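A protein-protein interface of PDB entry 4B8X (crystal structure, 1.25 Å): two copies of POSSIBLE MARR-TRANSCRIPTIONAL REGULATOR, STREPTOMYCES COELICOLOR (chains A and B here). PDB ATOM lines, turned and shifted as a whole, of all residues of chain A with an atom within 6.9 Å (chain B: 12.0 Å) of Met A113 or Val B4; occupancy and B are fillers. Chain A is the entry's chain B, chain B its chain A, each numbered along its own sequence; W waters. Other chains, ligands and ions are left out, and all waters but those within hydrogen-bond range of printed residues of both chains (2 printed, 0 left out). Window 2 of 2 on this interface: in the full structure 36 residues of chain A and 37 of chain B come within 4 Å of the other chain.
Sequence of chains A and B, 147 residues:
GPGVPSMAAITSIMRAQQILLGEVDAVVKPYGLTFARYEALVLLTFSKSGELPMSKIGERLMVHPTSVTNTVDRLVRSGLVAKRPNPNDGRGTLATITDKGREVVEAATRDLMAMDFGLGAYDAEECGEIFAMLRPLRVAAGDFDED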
ATOM      1  N   VAL A  27       2.536 -28.926   9.369  1.00  0.00           N
ATOM      2  CA  VAL A  27       1.505 -27.921   9.647  1.00  0.00           C
ATOM      3  C   VAL A  27       1.627 -26.708   8.725  1.00  0.00           C
ATOM      4  O   VAL A  27       0.616 -26.183   8.273  1.00  0.00           O
ATOM      5  CB  VAL A  27       1.531 -27.460  11.135  1.00  0.00           C
ATOM      6  CG1 VAL A  27       0.601 -26.281  11.357  1.00  0.00           C
ATOM      7  CG2 VAL A  27       1.146 -28.597  12.058  1.00  0.00           C
ATOM      8  N   TYR A  38       8.559 -19.766   8.193  1.00  0.00           N
ATOM      9  CA  TYR A  38       7.585 -19.281   9.161  1.00  0.00           C
ATOM     10  C   TYR A  38       8.227 -18.396  10.245  1.00  0.00           C
ATOM     11  O   TYR A  38       7.716 -17.329  10.541  1.00  0.00           O
ATOM     12  CB  TYR A  38       6.838 -20.478   9.764  1.00  0.00           C
ATOM     13  CG  TYR A  38       6.078 -20.119  10.997  1.00  0.00           C
ATOM     14  CD1 TYR A  38       4.842 -19.517  10.906  1.00  0.00           C
ATOM     15  CD2 TYR A  38       6.584 -20.387  12.280  1.00  0.00           C
ATOM     16  CE1 TYR A  38       4.132 -19.159  12.043  1.00  0.00           C
ATOM     17  CE2 TYR A  38       5.884 -20.029  13.422  1.00  0.00           C
ATOM     18  CZ  TYR A  38       4.659 -19.421  13.295  1.00  0.00           C
ATOM     19  OH  TYR A  38       3.950 -19.083  14.423  1.00  0.00           O
ATOM     20  N   ALA A 108      -1.044 -19.708  10.132  1.00  0.00           N
ATOM     21  CA  ALA A 108      -0.072 -20.737  10.475  1.00  0.00           C
ATOM     22  C   ALA A 108       0.151 -20.775  11.987  1.00  0.00           C
ATOM     23  O   ALA A 108       0.245 -21.854  12.582  1.00  0.00           O
ATOM     24  CB  ALA A 108       1.229 -20.521   9.740  1.00  0.00           C
ATOM     25  N   THR A 109       0.220 -19.603  12.617  1.00  0.00           N
ATOM     26  CA  THR A 109       0.404 -19.545  14.076  1.00  0.00           C
ATOM     27  C   THR A 109      -0.775 -20.197  14.804  1.00  0.00           C
ATOM     28  O   THR A 109      -0.585 -20.962  15.755  1.00  0.00           O
ATOM     29  CB  THR A 109       0.618 -18.109  14.577  1.00  0.00           C
ATOM     30  OG1 THR A 109       1.808 -17.582  13.984  1.00  0.00           O
ATOM     31  CG2 THR A 109       0.766 -18.071  16.096  1.00  0.00           C
ATOM     32  N   ARG A 110      -1.990 -19.895  14.362  1.00  0.00           N
ATOM     33  CA  ARG A 110      -3.161 -20.531  14.945  1.00  0.00           C
ATOM     34  C   ARG A 110      -3.087 -22.053  14.826  1.00  0.00           C
ATOM     35  O   ARG A 110      -3.350 -22.756  15.789  1.00  0.00           O
ATOM     36  CB  ARG A 110      -4.435 -20.020  14.257  1.00  0.00           C
ATOM     37  CG  ARG A 110      -5.711 -20.525  14.889  1.00  0.00           C
ATOM     38  N   ASP A 111      -2.726 -22.549  13.645  1.00  0.00           N
ATOM     39  CA  ASP A 111      -2.602 -23.986  13.407  1.00  0.00           C
ATOM     40  C   ASP A 111      -1.522 -24.612  14.302  1.00  0.00           C
ATOM     41  O   ASP A 111      -1.732 -25.686  14.850  1.00  0.00           O
ATOM     42  CB  ASP A 111      -2.283 -24.266  11.928  1.00  0.00           C
ATOM     43  CG  ASP A 111      -3.425 -23.933  10.984  1.00  0.00           C
ATOM     44  OD1 ASP A 111      -4.529 -23.598  11.437  1.00  0.00           O
ATOM     45  OD2 ASP A 111      -3.184 -24.003   9.756  1.00  0.00           O
ATOM     46  N   LEU A 112      -0.366 -23.957  14.414  1.00  0.00           N
ATOM     47  CA  LEU A 112       0.737 -24.471  15.244  1.00  0.00           C
ATOM     48  C   LEU A 112       0.370 -24.470  16.726  1.00  0.00           C
ATOM     49  O   LEU A 112       0.653 -25.431  17.452  1.00  0.00           O
ATOM     50  CB  LEU A 112       1.995 -23.644  15.008  1.00  0.00           C
ATOM     51  CG  LEU A 112       2.689 -23.866  13.645  1.00  0.00           C
ATOM     52  CD1 LEU A 112       3.601 -22.685  13.332  1.00  0.00           C
ATOM     53  CD2 LEU A 112       3.463 -25.177  13.661  1.00  0.00           C
ATOM     54  N   MET A 113      -0.254 -23.391  17.189  1.00  0.00           N
ATOM     55  CA  MET A 113      -0.724 -23.290  18.577  1.00  0.00           C
ATOM     56  C   MET A 113      -1.702 -24.421  18.905  1.00  0.00           C
ATOM     57  O   MET A 113      -1.649 -24.991  20.002  1.00  0.00           O
ATOM     58  CB  MET A 113      -1.393 -21.927  18.840  1.00  0.00           C
ATOM     59  CG  MET A 113      -0.473 -20.717  18.800  1.00  0.00           C
ATOM     60  SD  MET A 113       0.677 -20.530  20.184  1.00  0.00           S
ATOM     61  CE  MET A 113      -0.415 -20.097  21.535  1.00  0.00           C
ATOM     62  N   ALA A 114      -2.580 -24.738  17.949  1.00  0.00           N
ATOM     63  CA  ALA A 114      -3.586 -25.784  18.134  1.00  0.00           C
ATOM     64  C   ALA A 114      -2.977 -27.168  18.340  1.00  0.00           C
ATOM     65  O   ALA A 114      -3.625 -28.034  18.942  1.00  0.00           O
ATOM     66  CB  ALA A 114      -4.564 -25.807  16.962  1.00  0.00           C
ATOM     67  N   MET A 115      -1.767 -27.399  17.830  1.00  0.00           N
ATOM     68  CA  MET A 115      -1.078 -28.678  18.061  1.00  0.00           C
ATOM     69  C   MET A 115       0.133 -28.521  18.997  1.00  0.00           C
ATOM     70  O   MET A 115       0.959 -29.421  19.110  1.00  0.00           O
ATOM     71  CB  MET A 115      -0.725 -29.400  16.744  1.00  0.00           C
ATOM     72  CG  MET A 115      -0.088 -28.563  15.644  1.00  0.00           C
ATOM     73  SD  MET A 115       1.678 -28.241  15.848  1.00  0.00           S
ATOM     74  CE  MET A 115       2.397 -29.844  15.473  1.00  0.00           C
ATOM     75  N   ASP A 116       0.208 -27.389  19.719  1.00  0.00           N
ATOM     76  CA  ASP A 116       1.268 -27.148  20.706  1.00  0.00           C
ATOM     77  C   ASP A 116       2.676 -27.368  20.162  1.00  0.00           C
ATOM     78  O   ASP A 116       3.566 -27.845  20.881  1.00  0.00           O
ATOM     79  CB  ASP A 116       1.039 -28.040  21.935  1.00  0.00           C
ATOM     80  CG  ASP A 116      -0.338 -27.864  22.546  1.00  0.00           C
ATOM     81  OD1 ASP A 116      -0.650 -26.763  23.025  1.00  0.00           O
ATOM     82  OD2 ASP A 116      -1.139 -28.811  22.521  1.00  0.00           O
ATOM     83  N   PHE A 117       2.889 -27.001  18.904  1.00  0.00           N
ATOM     84  CA  PHE A 117       4.187 -27.127  18.268  1.00  0.00           C
ATOM     85  C   PHE A 117       4.777 -28.527  18.374  1.00  0.00           C
ATOM     86  O   PHE A 117       5.987 -28.688  18.429  1.00  0.00           O
ATOM     87  CB  PHE A 117       5.165 -26.048  18.804  1.00  0.00           C
ATOM     88  CG  PHE A 117       4.791 -24.642  18.394  1.00  0.00           C
ATOM     89  CD1 PHE A 117       3.835 -23.923  19.073  1.00  0.00           C
ATOM     90  CD2 PHE A 117       5.389 -24.048  17.311  1.00  0.00           C
ATOM     91  CE1 PHE A 117       3.478 -22.652  18.671  1.00  0.00           C
ATOM     92  CE2 PHE A 117       5.069 -22.758  16.929  1.00  0.00           C
ATOM     93  CZ  PHE A 117       4.110 -22.069  17.611  1.00  0.00           C
ATOM     94  N   CME A 127       7.692 -28.785  29.527  1.00  0.00           N
ATOM     95  CA  CME A 127       8.127 -27.775  28.553  1.00  0.00           C
ATOM     96  CB  CME A 127       6.906 -27.166  27.826  1.00  0.00           C
ATOM     97  SG  CME A 127       6.271 -28.271  26.567  1.00  0.00           S
ATOM     98  SD  CME A 127       4.563 -27.571  25.853  1.00  0.00           S
ATOM     99  CE  CME A 127       3.302 -28.538  26.625  1.00  0.00           C
ATOM    100  CZ  CME A 127       1.967 -27.784  26.619  1.00  0.00           C
ATOM    101  OH  CME A 127       2.013 -26.713  27.580  1.00  0.00           O
ATOM    102  C   CME A 127       9.003 -26.733  29.225  1.00  0.00           C
ATOM    103  O   CME A 127      10.008 -26.287  28.671  1.00  0.00           O
ATOM    104  N   GLY B   3       7.123 -16.931  27.673  1.00  0.00           N
ATOM    105  CA  GLY B   3       6.045 -16.916  26.623  1.00  0.00           C
ATOM    106  C   GLY B   3       5.047 -18.073  26.753  1.00  0.00           C
ATOM    107  O   GLY B   3       4.547 -18.353  27.837  1.00  0.00           O
ATOM    108  N   VAL B   4       4.698 -18.708  25.637  1.00  0.00           N
ATOM    109  CA  VAL B   4       3.864 -19.920  25.663  1.00  0.00           C
ATOM    110  C   VAL B   4       4.826 -21.116  25.874  1.00  0.00           C
ATOM    111  O   VAL B   4       5.839 -21.188  25.203  1.00  0.00           O
ATOM    112  CB  VAL B   4       3.152 -20.047  24.318  1.00  0.00           C
ATOM    113  CG1 VAL B   4       2.408 -21.359  24.192  1.00  0.00           C
ATOM    114  CG2 VAL B   4       2.214 -18.867  24.110  1.00  0.00           C
ATOM    115  N   PRO B   5       4.531 -22.058  26.809  1.00  0.00           N
ATOM    116  CA  PRO B   5       5.567 -23.105  27.091  1.00  0.00           C
ATOM    117  C   PRO B   5       6.014 -23.921  25.867  1.00  0.00           C
ATOM    118  O   PRO B   5       7.224 -24.159  25.705  1.00  0.00           O
ATOM    119  CB  PRO B   5       4.891 -23.984  28.142  1.00  0.00           C
ATOM    120  CG  PRO B   5       3.989 -23.005  28.873  1.00  0.00           C
ATOM    121  CD  PRO B   5       3.428 -22.142  27.779  1.00  0.00           C
ATOM    122  N   SER B   6       5.078 -24.303  25.014  1.00  0.00           N
ATOM    123  CA  SER B   6       5.464 -25.075  23.837  1.00  0.00           C
ATOM    124  C   SER B   6       6.371 -24.300  22.885  1.00  0.00           C
ATOM    125  O   SER B   6       7.267 -24.879  22.283  1.00  0.00           O
ATOM    126  CB  SER B   6       4.231 -25.593  23.121  1.00  0.00           C
ATOM    127  OG  SER B   6       3.489 -24.529  22.585  1.00  0.00           O
ATOM    128  N   MET B   7       6.113 -23.001  22.733  1.00  0.00           N
ATOM    129  CA  MET B   7       6.938 -22.119  21.893  1.00  0.00           C
ATOM    130  C   MET B   7       8.349 -22.028  22.457  1.00  0.00           C
ATOM    131  O   MET B   7       9.338 -22.134  21.713  1.00  0.00           O
ATOM    132  CB  MET B   7       6.357 -20.699  21.825  1.00  0.00           C
ATOM    133  CG  MET B   7       5.284 -20.489  20.773  1.00  0.00           C
ATOM    134  SD  MET B   7       4.804 -18.742  20.637  1.00  0.00           S
ATOM    135  CE  MET B   7       3.414 -18.829  19.520  1.00  0.00           C
ATOM    136  N   ALA B   8       8.459 -21.810  23.766  1.00  0.00           N
ATOM    137  CA  ALA B   8       9.754 -21.729  24.398  1.00  0.00           C
ATOM    138  C   ALA B   8      10.514 -23.029  24.256  1.00  0.00           C
ATOM    139  O   ALA B   8      11.725 -23.027  23.992  1.00  0.00           O
ATOM    140  CB  ALA B   8       9.573 -21.387  25.866  1.00  0.00           C
ATOM    141  N   ALA B   9       9.828 -24.158  24.425  1.00  0.00           N
ATOM    142  CA  ALA B   9      10.490 -25.464  24.362  1.00  0.00           C
ATOM    143  C   ALA B   9      10.958 -25.788  22.955  1.00  0.00           C
ATOM    144  O   ALA B   9      12.083 -26.229  22.759  1.00  0.00           O
ATOM    145  CB  ALA B   9       9.572 -26.533  24.923  1.00  0.00           C
ATOM    146  N   ILE B  10      10.097 -25.611  21.956  1.00  0.00           N
ATOM    147  CA  ILE B  10      10.518 -25.939  20.600  1.00  0.00           C
ATOM    148  C   ILE B  10      11.677 -25.049  20.156  1.00  0.00           C
ATOM    149  O   ILE B  10      12.610 -25.519  19.533  1.00  0.00           O
ATOM    150  CB  ILE B  10       9.348 -25.967  19.578  1.00  0.00           C
ATOM    151  CG1 ILE B  10       9.839 -26.606  18.270  1.00  0.00           C
ATOM    152  CG2 ILE B  10       8.764 -24.577  19.322  1.00  0.00           C
ATOM    153  CD1 ILE B  10       8.768 -26.883  17.248  1.00  0.00           C
ATOM    154  N   THR B  11      11.614 -23.761  20.473  1.00  0.00           N
ATOM    155  CA  THR B  11      12.705 -22.857  20.134  1.00  0.00           C
ATOM    156  C   THR B  11      14.004 -23.327  20.775  1.00  0.00           C
ATOM    157  O   THR B  11      15.083 -23.306  20.167  1.00  0.00           O
ATOM    158  CB  THR B  11      12.380 -21.395  20.525  1.00  0.00           C
ATOM    159  OG1 THR B  11      11.214 -20.989  19.811  1.00  0.00           O
ATOM    160  CG2 THR B  11      13.562 -20.470  20.208  1.00  0.00           C
ATOM    161  N   SER B  12      13.918 -23.703  22.040  1.00  0.00           N
ATOM    162  CA  SER B  12      15.086 -24.166  22.734  1.00  0.00           C
ATOM    163  C   SER B  12      15.720 -25.403  22.089  1.00  0.00           C
ATOM    164  O   SER B  12      16.944 -25.467  21.963  1.00  0.00           O
ATOM    165  CB  SER B  12      14.753 -24.511  24.199  1.00  0.00           C
ATOM    166  OG  SER B  12      14.271 -23.405  24.914  1.00  0.00           O
ATOM    167  N   ILE B  13      14.882 -26.373  21.717  1.00  0.00           N
ATOM    168  CA  ILE B  13      15.366 -27.591  21.076  1.00  0.00           C
ATOM    169  C   ILE B  13      15.982 -27.275  19.709  1.00  0.00           C
ATOM    170  O   ILE B  13      17.048 -27.803  19.373  1.00  0.00           O
ATOM    171  CB  ILE B  13      14.209 -28.619  20.971  1.00  0.00           C
ATOM    172  CG1 ILE B  13      13.870 -29.185  22.355  1.00  0.00           C
ATOM    173  CG2 ILE B  13      14.599 -29.725  20.005  1.00  0.00           C
ATOM    174  CD1 ILE B  13      12.519 -29.850  22.445  1.00  0.00           C
HETATM  175  O   HOH W   1       2.195 -24.636  25.697  1.00  0.00           O
HETATM  176  O   HOH W   2       0.870 -24.762  23.350  1.00  0.00           O
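SD of CME A127 lies close to the backbone NH of Ser B6.
The backbone carbonyl oxygen (O) of Met B7 is in hydrogen-bond range of the side-chain hydroxyl (OG1) of Thr B11, 2.9 Å away. N of Phe A117 is in hydrogen-bond range of O of Leu A112 (3.1 Å). The side-chain sulfur of Met A115 lies close to the backbone NH of Phe A117, at 3.5 Å.
Among the printed residues, merely in contact across the chains: Asp A116 with Ser B6 (3.2 Å), Met A113 with Met B7 (3.3 Å), Phe A117 with Met B7 (3.5 Å), Phe A117 with Ile B10 (3.5 Å), Phe A117 with Ser B6 (3.6 Å), CME A127 with Pro B5 (3.7 Å), CME A127 with Ala B9 (3.8 Å) and Met A113 with Val B4 (3.9 Å).
No residue of chain B comes within 4 Å of Leu A112. Of the printed residues of chain B, Met A113 touches Val B4 (3.9 Å) and Met B7 (3.3 Å). No residue of chain B comes within 4 Å of Ala A114. No residue of chain B comes within 4 Å of Met A115. Asp A116 touches just one residue of chain B: Ser B6. Printed residues of chain A within 4 Å of Val B4: Met A113 (3.9 Å). Of the printed residues of chain A, Ser B6 touches Asp A116 (3.2 Å), Phe A117 (3.6 Å) and CME A127 (3.3 Å). Of the printed residues of chain A, Ala B9 touches CME A127. Of the printed residues of chain A, Ile B10 touches Phe A117. The nearest printed residue of chain B that does not touch Met A113 is Ser B6 (5.4 Å). The nearest printed residue of chain A that does not touch Val B4 is Phe A117 (5.8 Å). The nearest printed residue of chain A that does not touch Ser B6 is Met A113 (5.4 Å).
Hydrophobic or aromatic side chains of chain A that line the printed part of chain B: Met A113 and Phe A117. Of the 11 printed residues of chain B, 6 touch a printed residue of chain A. Among the printed residues, no Asp or Glu carboxylate lies within 4 Å of a Lys or Arg side-chain nitrogen of the other chain.
No position is printed for both chains. Of the 9 pairs that touch across the chains among the printed residues, none has its exchanged pair printed and touching as well.
Water W2 bridges the side-chain carboxylate of Asp A116 (2.5 Å) and the side-chain hydroxyl of Ser B6 (2.7 Å). Water W1 lies within hydrogen-bond range of OH of CME A127 and the backbone NH of Ser B6.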
